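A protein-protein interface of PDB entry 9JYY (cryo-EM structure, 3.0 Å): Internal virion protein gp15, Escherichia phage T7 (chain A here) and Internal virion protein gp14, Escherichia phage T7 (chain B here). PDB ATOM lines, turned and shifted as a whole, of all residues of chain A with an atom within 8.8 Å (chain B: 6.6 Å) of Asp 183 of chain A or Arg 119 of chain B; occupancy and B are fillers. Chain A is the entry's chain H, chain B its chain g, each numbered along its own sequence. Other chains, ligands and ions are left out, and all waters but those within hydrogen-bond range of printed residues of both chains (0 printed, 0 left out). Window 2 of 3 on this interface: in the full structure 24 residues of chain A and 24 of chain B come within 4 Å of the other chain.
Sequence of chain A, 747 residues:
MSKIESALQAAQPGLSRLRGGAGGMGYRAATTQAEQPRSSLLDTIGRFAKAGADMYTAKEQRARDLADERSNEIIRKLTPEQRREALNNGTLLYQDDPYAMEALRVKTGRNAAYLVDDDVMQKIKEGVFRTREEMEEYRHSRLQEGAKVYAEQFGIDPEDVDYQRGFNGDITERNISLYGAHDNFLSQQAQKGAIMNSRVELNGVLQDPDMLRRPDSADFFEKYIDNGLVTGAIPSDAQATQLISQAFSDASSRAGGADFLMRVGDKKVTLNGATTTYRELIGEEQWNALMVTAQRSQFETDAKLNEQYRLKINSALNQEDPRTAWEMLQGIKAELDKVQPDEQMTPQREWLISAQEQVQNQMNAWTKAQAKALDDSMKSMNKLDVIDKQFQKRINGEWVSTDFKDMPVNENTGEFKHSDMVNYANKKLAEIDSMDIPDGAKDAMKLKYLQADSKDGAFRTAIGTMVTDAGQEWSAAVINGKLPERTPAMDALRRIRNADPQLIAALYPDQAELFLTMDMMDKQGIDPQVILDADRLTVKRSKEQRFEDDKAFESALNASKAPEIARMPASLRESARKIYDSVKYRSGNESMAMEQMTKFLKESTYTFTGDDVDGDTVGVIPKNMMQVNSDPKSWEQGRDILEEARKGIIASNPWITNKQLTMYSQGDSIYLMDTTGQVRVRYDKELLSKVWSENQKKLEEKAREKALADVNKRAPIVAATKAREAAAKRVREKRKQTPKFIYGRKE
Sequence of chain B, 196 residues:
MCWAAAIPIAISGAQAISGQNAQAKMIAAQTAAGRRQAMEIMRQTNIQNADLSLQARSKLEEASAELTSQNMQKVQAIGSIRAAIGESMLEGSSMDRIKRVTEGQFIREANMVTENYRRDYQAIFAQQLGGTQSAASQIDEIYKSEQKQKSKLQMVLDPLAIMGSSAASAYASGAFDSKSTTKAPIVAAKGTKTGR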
ATOM      1  N   GLN A 122      12.080 -40.097  25.552  1.00  0.00           N
ATOM      2  CA  GLN A 122      12.827 -38.916  25.137  1.00  0.00           C
ATOM      3  C   GLN A 122      13.667 -39.194  23.901  1.00  0.00           C
ATOM      4  O   GLN A 122      13.748 -38.355  22.993  1.00  0.00           O
ATOM      5  CB  GLN A 122      13.714 -38.435  26.278  1.00  0.00           C
ATOM      6  CG  GLN A 122      14.257 -37.052  26.068  1.00  0.00           C
ATOM      7  CD  GLN A 122      13.187 -36.012  26.182  1.00  0.00           C
ATOM      8  OE1 GLN A 122      12.607 -35.605  25.183  1.00  0.00           O
ATOM      9  NE2 GLN A 122      12.911 -35.575  27.401  1.00  0.00           N
ATOM     10  N   LYS A 125      11.352 -39.097  21.103  1.00  0.00           N
ATOM     11  CA  LYS A 125      10.973 -37.708  20.848  1.00  0.00           C
ATOM     12  C   LYS A 125      12.034 -36.960  20.063  1.00  0.00           C
ATOM     13  O   LYS A 125      11.705 -36.060  19.286  1.00  0.00           O
ATOM     14  CB  LYS A 125      10.751 -36.948  22.148  1.00  0.00           C
ATOM     15  CG  LYS A 125       9.593 -37.322  23.009  1.00  0.00           C
ATOM     16  CD  LYS A 125       9.642 -36.362  24.165  1.00  0.00           C
ATOM     17  CE  LYS A 125       8.587 -36.640  25.176  1.00  0.00           C
ATOM     18  NZ  LYS A 125       7.256 -36.363  24.634  1.00  0.00           N
ATOM     19  N   PHE A 129       8.354 -38.288  16.825  1.00  0.00           N
ATOM     20  CA  PHE A 129       6.938 -38.004  17.061  1.00  0.00           C
ATOM     21  C   PHE A 129       6.529 -36.767  16.282  1.00  0.00           C
ATOM     22  O   PHE A 129       6.999 -35.661  16.566  1.00  0.00           O
ATOM     23  CB  PHE A 129       6.585 -37.836  18.537  1.00  0.00           C
ATOM     24  CG  PHE A 129       6.713 -39.088  19.325  1.00  0.00           C
ATOM     25  CD1 PHE A 129       5.710 -40.034  19.284  1.00  0.00           C
ATOM     26  CD2 PHE A 129       7.805 -39.319  20.125  1.00  0.00           C
ATOM     27  CE1 PHE A 129       5.810 -41.202  19.998  1.00  0.00           C
ATOM     28  CE2 PHE A 129       7.897 -40.481  20.861  1.00  0.00           C
ATOM     29  CZ  PHE A 129       6.906 -41.429  20.785  1.00  0.00           C
ATOM     30  N   THR A 131       3.405 -35.434  16.249  1.00  0.00           N
ATOM     31  CA  THR A 131       2.495 -34.599  17.013  1.00  0.00           C
ATOM     32  C   THR A 131       2.378 -35.119  18.439  1.00  0.00           C
ATOM     33  O   THR A 131       2.787 -36.237  18.757  1.00  0.00           O
ATOM     34  CB  THR A 131       1.108 -34.533  16.356  1.00  0.00           C
ATOM     35  OG1 THR A 131       0.308 -33.546  17.015  1.00  0.00           O
ATOM     36  CG2 THR A 131       0.412 -35.877  16.443  1.00  0.00           C
ATOM     37  N   ARG A 132       1.803 -34.274  19.295  1.00  0.00           N
ATOM     38  CA  ARG A 132       1.699 -34.592  20.714  1.00  0.00           C
ATOM     39  C   ARG A 132       0.744 -35.754  20.962  1.00  0.00           C
ATOM     40  O   ARG A 132       0.883 -36.479  21.954  1.00  0.00           O
ATOM     41  CB  ARG A 132       1.240 -33.355  21.480  1.00  0.00           C
ATOM     42  CG  ARG A 132       1.066 -33.568  22.963  1.00  0.00           C
ATOM     43  CD  ARG A 132       0.858 -32.254  23.687  1.00  0.00           C
ATOM     44  NE  ARG A 132       2.021 -31.384  23.616  1.00  0.00           N
ATOM     45  CZ  ARG A 132       2.178 -30.297  24.359  1.00  0.00           C
ATOM     46  NH1 ARG A 132       1.267 -29.930  25.244  1.00  0.00           N
ATOM     47  NH2 ARG A 132       3.277 -29.564  24.213  1.00  0.00           N
ATOM     48  N   MET A 135       2.436 -38.997  20.653  1.00  0.00           N
ATOM     49  CA  MET A 135       3.316 -38.961  21.814  1.00  0.00           C
ATOM     50  C   MET A 135       2.627 -39.485  23.066  1.00  0.00           C
ATOM     51  O   MET A 135       3.152 -40.376  23.747  1.00  0.00           O
ATOM     52  CB  MET A 135       3.788 -37.527  22.026  1.00  0.00           C
ATOM     53  CG  MET A 135       5.139 -37.364  22.632  1.00  0.00           C
ATOM     54  SD  MET A 135       4.934 -37.448  24.424  1.00  0.00           S
ATOM     55  CE  MET A 135       4.138 -35.877  24.771  1.00  0.00           C
ATOM     56  N   ASN A 175       6.432 -35.021  33.180  1.00  0.00           N
ATOM     57  CA  ASN A 175       5.565 -34.608  32.086  1.00  0.00           C
ATOM     58  C   ASN A 175       5.965 -33.238  31.571  1.00  0.00           C
ATOM     59  O   ASN A 175       5.968 -32.997  30.362  1.00  0.00           O
ATOM     60  CB  ASN A 175       4.111 -34.593  32.547  1.00  0.00           C
ATOM     61  CG  ASN A 175       3.490 -35.967  32.550  1.00  0.00           C
ATOM     62  OD1 ASN A 175       3.961 -36.874  31.870  1.00  0.00           O
ATOM     63  ND2 ASN A 175       2.422 -36.128  33.317  1.00  0.00           N
ATOM     64  N   ILE A 176       6.296 -32.325  32.481  1.00  0.00           N
ATOM     65  CA  ILE A 176       6.754 -31.003  32.069  1.00  0.00           C
ATOM     66  C   ILE A 176       7.973 -31.127  31.167  1.00  0.00           C
ATOM     67  O   ILE A 176       8.019 -30.553  30.075  1.00  0.00           O
ATOM     68  CB  ILE A 176       7.054 -30.126  33.294  1.00  0.00           C
ATOM     69  CG1 ILE A 176       5.758 -29.777  34.022  1.00  0.00           C
ATOM     70  CG2 ILE A 176       7.786 -28.877  32.875  1.00  0.00           C
ATOM     71  CD1 ILE A 176       5.973 -29.188  35.390  1.00  0.00           C
ATOM     72  N   SER A 177       8.965 -31.906  31.598  1.00  0.00           N
ATOM     73  CA  SER A 177      10.178 -32.059  30.804  1.00  0.00           C
ATOM     74  C   SER A 177       9.882 -32.685  29.448  1.00  0.00           C
ATOM     75  O   SER A 177      10.375 -32.212  28.418  1.00  0.00           O
ATOM     76  CB  SER A 177      11.199 -32.899  31.564  1.00  0.00           C
ATOM     77  OG  SER A 177      12.240 -33.316  30.703  1.00  0.00           O
ATOM     78  N   LEU A 178       9.076 -33.748  29.422  1.00  0.00           N
ATOM     79  CA  LEU A 178       8.845 -34.465  28.170  1.00  0.00           C
ATOM     80  C   LEU A 178       8.043 -33.627  27.185  1.00  0.00           C
ATOM     81  O   LEU A 178       8.372 -33.567  25.993  1.00  0.00           O
ATOM     82  CB  LEU A 178       8.132 -35.783  28.447  1.00  0.00           C
ATOM     83  CG  LEU A 178       8.948 -36.838  29.186  1.00  0.00           C
ATOM     84  CD1 LEU A 178       8.002 -37.720  29.930  1.00  0.00           C
ATOM     85  CD2 LEU A 178       9.818 -37.663  28.263  1.00  0.00           C
ATOM     86  N   TYR A 179       6.982 -32.977  27.661  1.00  0.00           N
ATOM     87  CA  TYR A 179       6.191 -32.132  26.780  1.00  0.00           C
ATOM     88  C   TYR A 179       6.992 -30.926  26.321  1.00  0.00           C
ATOM     89  O   TYR A 179       6.863 -30.500  25.173  1.00  0.00           O
ATOM     90  CB  TYR A 179       4.902 -31.703  27.472  1.00  0.00           C
ATOM     91  CG  TYR A 179       3.838 -32.774  27.444  1.00  0.00           C
ATOM     92  CD1 TYR A 179       4.025 -33.981  28.099  1.00  0.00           C
ATOM     93  CD2 TYR A 179       2.665 -32.594  26.740  1.00  0.00           C
ATOM     94  CE1 TYR A 179       3.064 -34.963  28.068  1.00  0.00           C
ATOM     95  CE2 TYR A 179       1.698 -33.573  26.702  1.00  0.00           C
ATOM     96  CZ  TYR A 179       1.902 -34.754  27.364  1.00  0.00           C
ATOM     97  OH  TYR A 179       0.939 -35.734  27.329  1.00  0.00           O
ATOM     98  N   GLY A 180       7.845 -30.376  27.187  1.00  0.00           N
ATOM     99  CA  GLY A 180       8.711 -29.294  26.757  1.00  0.00           C
ATOM    100  C   GLY A 180       9.714 -29.733  25.711  1.00  0.00           C
ATOM    101  O   GLY A 180      10.058 -28.971  24.808  1.00  0.00           O
ATOM    102  N   ALA A 181      10.203 -30.966  25.819  1.00  0.00           N
ATOM    103  CA  ALA A 181      11.152 -31.461  24.832  1.00  0.00           C
ATOM    104  C   ALA A 181      10.477 -31.688  23.487  1.00  0.00           C
ATOM    105  O   ALA A 181      11.031 -31.336  22.440  1.00  0.00           O
ATOM    106  CB  ALA A 181      11.803 -32.742  25.337  1.00  0.00           C
ATOM    107  N   HIS A 182       9.275 -32.264  23.493  1.00  0.00           N
ATOM    108  CA  HIS A 182       8.508 -32.356  22.254  1.00  0.00           C
ATOM    109  C   HIS A 182       8.212 -30.975  21.694  1.00  0.00           C
ATOM    110  O   HIS A 182       8.209 -30.768  20.474  1.00  0.00           O
ATOM    111  CB  HIS A 182       7.205 -33.111  22.485  1.00  0.00           C
ATOM    112  CG  HIS A 182       6.452 -33.397  21.225  1.00  0.00           C
ATOM    113  ND1 HIS A 182       6.889 -34.305  20.287  1.00  0.00           N
ATOM    114  CD2 HIS A 182       5.305 -32.873  20.737  1.00  0.00           C
ATOM    115  CE1 HIS A 182       6.035 -34.340  19.281  1.00  0.00           C
ATOM    116  NE2 HIS A 182       5.066 -33.479  19.528  1.00  0.00           N
ATOM    117  N   ASP A 183       7.948 -30.019  22.579  1.00  0.00           N
ATOM    118  CA  ASP A 183       7.656 -28.660  22.158  1.00  0.00           C
ATOM    119  C   ASP A 183       8.860 -28.028  21.470  1.00  0.00           C
ATOM    120  O   ASP A 183       8.724 -27.402  20.412  1.00  0.00           O
ATOM    121  CB  ASP A 183       7.236 -27.858  23.385  1.00  0.00           C
ATOM    122  CG  ASP A 183       6.654 -26.529  23.035  1.00  0.00           C
ATOM    123  OD1 ASP A 183       6.589 -26.217  21.830  1.00  0.00           O
ATOM    124  OD2 ASP A 183       6.260 -25.798  23.967  1.00  0.00           O
ATOM    125  N   ASN A 184      10.050 -28.194  22.050  1.00  0.00           N
ATOM    126  CA  ASN A 184      11.262 -27.714  21.395  1.00  0.00           C
ATOM    127  C   ASN A 184      11.508 -28.451  20.090  1.00  0.00           C
ATOM    128  O   ASN A 184      12.051 -27.879  19.142  1.00  0.00           O
ATOM    129  CB  ASN A 184      12.475 -27.852  22.314  1.00  0.00           C
ATOM    130  CG  ASN A 184      12.438 -26.887  23.474  1.00  0.00           C
ATOM    131  OD1 ASN A 184      12.081 -25.723  23.313  1.00  0.00           O
ATOM    132  ND2 ASN A 184      12.835 -27.360  24.650  1.00  0.00           N
ATOM    133  N   PHE A 185      11.127 -29.727  20.020  1.00  0.00           N
ATOM    134  CA  PHE A 185      11.243 -30.442  18.754  1.00  0.00           C
ATOM    135  C   PHE A 185      10.397 -29.788  17.673  1.00  0.00           C
ATOM    136  O   PHE A 185      10.861 -29.586  16.546  1.00  0.00           O
ATOM    137  CB  PHE A 185      10.822 -31.896  18.921  1.00  0.00           C
ATOM    138  CG  PHE A 185      10.674 -32.618  17.621  1.00  0.00           C
ATOM    139  CD1 PHE A 185      11.787 -33.018  16.910  1.00  0.00           C
ATOM    140  CD2 PHE A 185       9.423 -32.864  17.088  1.00  0.00           C
ATOM    141  CE1 PHE A 185      11.656 -33.668  15.709  1.00  0.00           C
ATOM    142  CE2 PHE A 185       9.286 -33.513  15.886  1.00  0.00           C
ATOM    143  CZ  PHE A 185      10.404 -33.915  15.196  1.00  0.00           C
ATOM    144  N   LEU A 186       9.146 -29.465  17.995  1.00  0.00           N
ATOM    145  CA  LEU A 186       8.289 -28.806  17.015  1.00  0.00           C
ATOM    146  C   LEU A 186       8.828 -27.430  16.655  1.00  0.00           C
ATOM    147  O   LEU A 186       8.761 -27.011  15.492  1.00  0.00           O
ATOM    148  CB  LEU A 186       6.860 -28.701  17.539  1.00  0.00           C
ATOM    149  CG  LEU A 186       6.072 -30.003  17.635  1.00  0.00           C
ATOM    150  CD1 LEU A 186       4.632 -29.699  17.969  1.00  0.00           C
ATOM    151  CD2 LEU A 186       6.165 -30.791  16.347  1.00  0.00           C
ATOM    152  N   SER A 187       9.359 -26.710  17.642  1.00  0.00           N
ATOM    153  CA  SER A 187       9.954 -25.405  17.375  1.00  0.00           C
ATOM    154  C   SER A 187      11.116 -25.529  16.403  1.00  0.00           C
ATOM    155  O   SER A 187      11.233 -24.752  15.449  1.00  0.00           O
ATOM    156  CB  SER A 187      10.417 -24.771  18.684  1.00  0.00           C
ATOM    157  OG  SER A 187      11.136 -23.577  18.441  1.00  0.00           O
ATOM    158  N   GLN A 188      11.985 -26.513  16.630  1.00  0.00           N
ATOM    159  CA  GLN A 188      13.106 -26.745  15.732  1.00  0.00           C
ATOM    160  C   GLN A 188      12.623 -27.111  14.341  1.00  0.00           C
ATOM    161  O   GLN A 188      13.159 -26.617  13.349  1.00  0.00           O
ATOM    162  CB  GLN A 188      14.007 -27.843  16.289  1.00  0.00           C
ATOM    163  CG  GLN A 188      14.781 -27.429  17.513  1.00  0.00           C
ATOM    164  CD  GLN A 188      15.592 -26.180  17.274  1.00  0.00           C
ATOM    165  OE1 GLN A 188      16.436 -26.141  16.381  1.00  0.00           O
ATOM    166  NE2 GLN A 188      15.340 -25.149  18.070  1.00  0.00           N
ATOM    167  N   GLN A 189      11.618 -27.980  14.248  1.00  0.00           N
ATOM    168  CA  GLN A 189      11.115 -28.389  12.942  1.00  0.00           C
ATOM    169  C   GLN A 189      10.588 -27.192  12.163  1.00  0.00           C
ATOM    170  O   GLN A 189      10.895 -27.025  10.974  1.00  0.00           O
ATOM    171  CB  GLN A 189      10.020 -29.439  13.114  1.00  0.00           C
ATOM    172  CG  GLN A 189       9.542 -30.060  11.824  1.00  0.00           C
ATOM    173  CD  GLN A 189       8.283 -30.876  12.008  1.00  0.00           C
ATOM    174  OE1 GLN A 189       7.509 -30.640  12.933  1.00  0.00           O
ATOM    175  NE2 GLN A 189       8.068 -31.841  11.122  1.00  0.00           N
ATOM    176  N   ALA A 190       9.811 -26.336  12.829  1.00  0.00           N
ATOM    177  CA  ALA A 190       9.299 -25.141  12.171  1.00  0.00           C
ATOM    178  C   ALA A 190      10.432 -24.216  11.752  1.00  0.00           C
ATOM    179  O   ALA A 190      10.396 -23.639  10.661  1.00  0.00           O
ATOM    180  CB  ALA A 190       8.325 -24.412  13.093  1.00  0.00           C
ATOM    181  N   GLN A 191      11.445 -24.059  12.604  1.00  0.00           N
ATOM    182  CA  GLN A 191      12.555 -23.181  12.255  1.00  0.00           C
ATOM    183  C   GLN A 191      13.323 -23.701  11.047  1.00  0.00           C
ATOM    184  O   GLN A 191      13.682 -22.926  10.155  1.00  0.00           O
ATOM    185  CB  GLN A 191      13.478 -23.003  13.457  1.00  0.00           C
ATOM    186  CG  GLN A 191      12.902 -22.082  14.509  1.00  0.00           C
ATOM    187  CD  GLN A 191      13.761 -21.982  15.743  1.00  0.00           C
ATOM    188  OE1 GLN A 191      14.695 -22.756  15.929  1.00  0.00           O
ATOM    189  NE2 GLN A 191      13.459 -21.012  16.590  1.00  0.00           N
ATOM    190  N   ASN B 111       7.084 -23.422  36.464  1.00  0.00           N
ATOM    191  CA  ASN B 111       7.635 -23.603  35.131  1.00  0.00           C
ATOM    192  C   ASN B 111       6.868 -22.819  34.081  1.00  0.00           C
ATOM    193  O   ASN B 111       7.169 -22.940  32.890  1.00  0.00           O
ATOM    194  CB  ASN B 111       7.656 -25.086  34.757  1.00  0.00           C
ATOM    195  CG  ASN B 111       8.551 -25.903  35.659  1.00  0.00           C
ATOM    196  OD1 ASN B 111       8.518 -27.129  35.633  1.00  0.00           O
ATOM    197  ND2 ASN B 111       9.363 -25.228  36.459  1.00  0.00           N
ATOM    198  N   MET B 112       5.882 -22.023  34.498  1.00  0.00           N
ATOM    199  CA  MET B 112       5.060 -21.229  33.589  1.00  0.00           C
ATOM    200  C   MET B 112       4.388 -22.123  32.549  1.00  0.00           C
ATOM    201  O   MET B 112       4.507 -21.918  31.341  1.00  0.00           O
ATOM    202  CB  MET B 112       5.888 -20.127  32.927  1.00  0.00           C
ATOM    203  CG  MET B 112       6.127 -18.928  33.823  1.00  0.00           C
ATOM    204  SD  MET B 112       7.832 -18.350  33.774  1.00  0.00           S
ATOM    205  CE  MET B 112       8.664 -19.649  34.683  1.00  0.00           C
ATOM    206  N   VAL B 113       3.681 -23.138  33.039  1.00  0.00           N
ATOM    207  CA  VAL B 113       3.078 -24.165  32.204  1.00  0.00           C
ATOM    208  C   VAL B 113       1.630 -24.368  32.625  1.00  0.00           C
ATOM    209  O   VAL B 113       1.308 -24.387  33.817  1.00  0.00           O
ATOM    210  CB  VAL B 113       3.871 -25.486  32.293  1.00  0.00           C
ATOM    211  CG1 VAL B 113       3.186 -26.564  31.519  1.00  0.00           C
ATOM    212  CG2 VAL B 113       5.277 -25.294  31.759  1.00  0.00           C
ATOM    213  N   THR B 114       0.751 -24.508  31.637  1.00  0.00           N
ATOM    214  CA  THR B 114      -0.666 -24.721  31.891  1.00  0.00           C
ATOM    215  C   THR B 114      -0.938 -26.187  32.221  1.00  0.00           C
ATOM    216  O   THR B 114      -0.037 -27.030  32.231  1.00  0.00           O
ATOM    217  CB  THR B 114      -1.495 -24.281  30.689  1.00  0.00           C
ATOM    218  OG1 THR B 114      -1.206 -25.127  29.571  1.00  0.00           O
ATOM    219  CG2 THR B 114      -1.177 -22.850  30.324  1.00  0.00           C
ATOM    220  N   TYR B 117      -0.082 -28.621  29.646  1.00  0.00           N
ATOM    221  CA  TYR B 117       1.362 -28.583  29.442  1.00  0.00           C
ATOM    222  C   TYR B 117       1.739 -27.740  28.234  1.00  0.00           C
ATOM    223  O   TYR B 117       2.873 -27.833  27.748  1.00  0.00           O
ATOM    224  CB  TYR B 117       1.971 -29.983  29.333  1.00  0.00           C
ATOM    225  CG  TYR B 117       1.893 -30.729  30.641  1.00  0.00           C
ATOM    226  CD1 TYR B 117       2.514 -30.232  31.776  1.00  0.00           C
ATOM    227  CD2 TYR B 117       1.173 -31.907  30.752  1.00  0.00           C
ATOM    228  CE1 TYR B 117       2.439 -30.897  32.977  1.00  0.00           C
ATOM    229  CE2 TYR B 117       1.091 -32.576  31.953  1.00  0.00           C
ATOM    230  CZ  TYR B 117       1.727 -32.067  33.061  1.00  0.00           C
ATOM    231  OH  TYR B 117       1.648 -32.732  34.259  1.00  0.00           O
ATOM    232  N   ARG B 118       0.820 -26.927  27.728  1.00  0.00           N
ATOM    233  CA  ARG B 118       1.179 -25.865  26.803  1.00  0.00           C
ATOM    234  C   ARG B 118       1.785 -24.703  27.577  1.00  0.00           C
ATOM    235  O   ARG B 118       1.424 -24.453  28.729  1.00  0.00           O
ATOM    236  CB  ARG B 118      -0.054 -25.408  26.028  1.00  0.00           C
ATOM    237  CG  ARG B 118       0.220 -24.971  24.605  1.00  0.00           C
ATOM    238  CD  ARG B 118       0.329 -26.159  23.675  1.00  0.00           C
ATOM    239  NE  ARG B 118      -0.896 -26.948  23.647  1.00  0.00           N
ATOM    240  CZ  ARG B 118      -1.003 -28.137  23.073  1.00  0.00           C
ATOM    241  NH1 ARG B 118       0.022 -28.702  22.456  1.00  0.00           N
ATOM    242  NH2 ARG B 118      -2.170 -28.773  23.111  1.00  0.00           N
ATOM    243  N   ARG B 119       2.713 -23.992  26.943  1.00  0.00           N
ATOM    244  CA  ARG B 119       3.364 -22.869  27.608  1.00  0.00           C
ATOM    245  C   ARG B 119       2.349 -21.792  27.970  1.00  0.00           C
ATOM    246  O   ARG B 119       1.512 -21.402  27.153  1.00  0.00           O
ATOM    247  CB  ARG B 119       4.448 -22.275  26.713  1.00  0.00           C
ATOM    248  CG  ARG B 119       5.725 -23.080  26.656  1.00  0.00           C
ATOM    249  CD  ARG B 119       6.844 -22.251  26.070  1.00  0.00           C
ATOM    250  NE  ARG B 119       8.110 -22.970  26.046  1.00  0.00           N
ATOM    251  CZ  ARG B 119       9.249 -22.455  25.610  1.00  0.00           C
ATOM    252  NH1 ARG B 119       9.321 -21.212  25.167  1.00  0.00           N
ATOM    253  NH2 ARG B 119      10.344 -23.208  25.616  1.00  0.00           N
ATOM    254  N   ASP B 120       2.434 -21.308  29.207  1.00  0.00           N
ATOM    255  CA  ASP B 120       1.557 -20.251  29.705  1.00  0.00           C
ATOM    256  C   ASP B 120       2.240 -18.914  29.452  1.00  0.00           C
ATOM    257  O   ASP B 120       3.028 -18.445  30.275  1.00  0.00           O
ATOM    258  CB  ASP B 120       1.259 -20.444  31.187  1.00  0.00           C
ATOM    259  CG  ASP B 120       0.273 -19.426  31.714  1.00  0.00           C
ATOM    260  OD1 ASP B 120      -0.647 -19.048  30.962  1.00  0.00           O
ATOM    261  OD2 ASP B 120       0.422 -18.996  32.877  1.00  0.00           O
ATOM    262  N   TYR B 121       1.929 -18.293  28.315  1.00  0.00           N
ATOM    263  CA  TYR B 121       2.617 -17.068  27.934  1.00  0.00           C
ATOM    264  C   TYR B 121       2.184 -15.859  28.748  1.00  0.00           C
ATOM    265  O   TYR B 121       2.960 -14.906  28.869  1.00  0.00           O
ATOM    266  CB  TYR B 121       2.409 -16.787  26.449  1.00  0.00           C
ATOM    267  CG  TYR B 121       3.155 -17.749  25.568  1.00  0.00           C
ATOM    268  CD1 TYR B 121       4.538 -17.792  25.576  1.00  0.00           C
ATOM    269  CD2 TYR B 121       2.478 -18.625  24.742  1.00  0.00           C
ATOM    270  CE1 TYR B 121       5.224 -18.672  24.777  1.00  0.00           C
ATOM    271  CE2 TYR B 121       3.156 -19.507  23.942  1.00  0.00           C
ATOM    272  CZ  TYR B 121       4.528 -19.528  23.963  1.00  0.00           C
ATOM    273  OH  TYR B 121       5.209 -20.411  23.164  1.00  0.00           O
ATOM    274  N   GLN B 122       0.972 -15.874  29.306  1.00  0.00           N
ATOM    275  CA  GLN B 122       0.522 -14.739  30.102  1.00  0.00           C
ATOM    276  C   GLN B 122       1.435 -14.517  31.299  1.00  0.00           C
ATOM    277  O   GLN B 122       1.817 -13.380  31.596  1.00  0.00           O
ATOM    278  CB  GLN B 122      -0.918 -14.956  30.560  1.00  0.00           C
ATOM    279  CG  GLN B 122      -1.949 -14.276  29.685  1.00  0.00           C
ATOM    280  CD  GLN B 122      -2.023 -12.783  29.928  1.00  0.00           C
ATOM    281  OE1 GLN B 122      -1.441 -12.267  30.882  1.00  0.00           O
ATOM    282  NE2 GLN B 122      -2.744 -12.077  29.064  1.00  0.00           N
ATOM    283  N   ILE B 124       4.491 -15.682  31.350  1.00  0.00           N
ATOM    284  CA  ILE B 124       5.800 -15.418  30.760  1.00  0.00           C
ATOM    285  C   ILE B 124       5.917 -13.957  30.344  1.00  0.00           C
ATOM    286  O   ILE B 124       6.922 -13.293  30.628  1.00  0.00           O
ATOM    287  CB  ILE B 124       6.051 -16.360  29.569  1.00  0.00           C
ATOM    288  CG1 ILE B 124       6.085 -17.813  30.027  1.00  0.00           C
ATOM    289  CG2 ILE B 124       7.356 -16.020  28.912  1.00  0.00           C
ATOM    290  CD1 ILE B 124       6.069 -18.802  28.888  1.00  0.00           C
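The side-chain carboxylate of Asp 183 of chain A is in salt-bridge range of the guanidinium group of Arg 119 of chain B, at 3.97 Å. NH1 of Arg 118 of chain B sits close to NH1 of Arg 132 of chain A (3.3 Å).
The backbone carbonyl oxygen (O) of Arg 118 of chain B is in hydrogen-bond range of the side-chain hydroxyl (OG1) of Thr 114 of chain B (2.8 Å). The backbone NH (N) of Arg 132 of chain A lies within hydrogen-bond range of a ring nitrogen (NE2) of His 182 of chain A, 3.4 Å away. O of Gly 180 of chain A sits at hydrogen-bond distance from ND2 of Asn 184 of chain A (3.2 Å).
Among the printed residues, pairs that only touch across the chains: Ile 176 of chain A with Asn 111 of chain B (3.3 Å), Asn 175 of chain A with Tyr 117 of chain B (3.5 Å), Arg 132 of chain A with Tyr 117 of chain B (3.6 Å), Ile 176 of chain A with Tyr 117 of chain B (3.7 Å), Tyr 179 of chain A with Tyr 117 of chain B (3.7 Å) and Asn 184 of chain A with Arg 119 of chain B (3.8 Å).
Of chain B, only Arg 119 (3.9 Å) comes within 4 Å of Asp 183 of chain A. Arg 119 of chain B touches just these residues of chain A: Asp 183 and Asn 184. Printed residues of chain B within 4 Å of Tyr 179 of chain A: Tyr 117 (3.7 Å). Printed residues of chain A within 4 Å of Tyr 117 of chain B: Arg 132 (3.6 Å), Asn 175 (3.5 Å), Ile 176 (3.7 Å) and Tyr 179 (3.7 Å). Printed residues of chain B within 4 Å of Ile 176 of chain A: Asn 111 and Tyr 117. Printed residues of chain A within 4 Å of Arg 118 of chain B: Arg 132 (3.3 Å). Printed residues of chain A within 4 Å of Asn 111 of chain B: Ile 176 (3.3 Å). Leu 186 of chain A touches none of the printed residues of chain B. The nearest residue of chain B that does not touch Asp 183 of chain A is Tyr 117 of chain B (5.5 Å). The nearest printed residue of chain A that does not touch Tyr 117 of chain B is Asp 183 of chain A (5.5 Å).
Of the 11 printed residues of chain B, 4 touch a printed residue of chain A. Hydrophobic or aromatic side chains of chain B that line the printed part of chain A: Tyr 117. Hydrophobic or aromatic side chains of chain A that line the printed part of chain B: Ile 176 and Tyr 179. Among the printed residues, 8 pairs touch across the chains.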
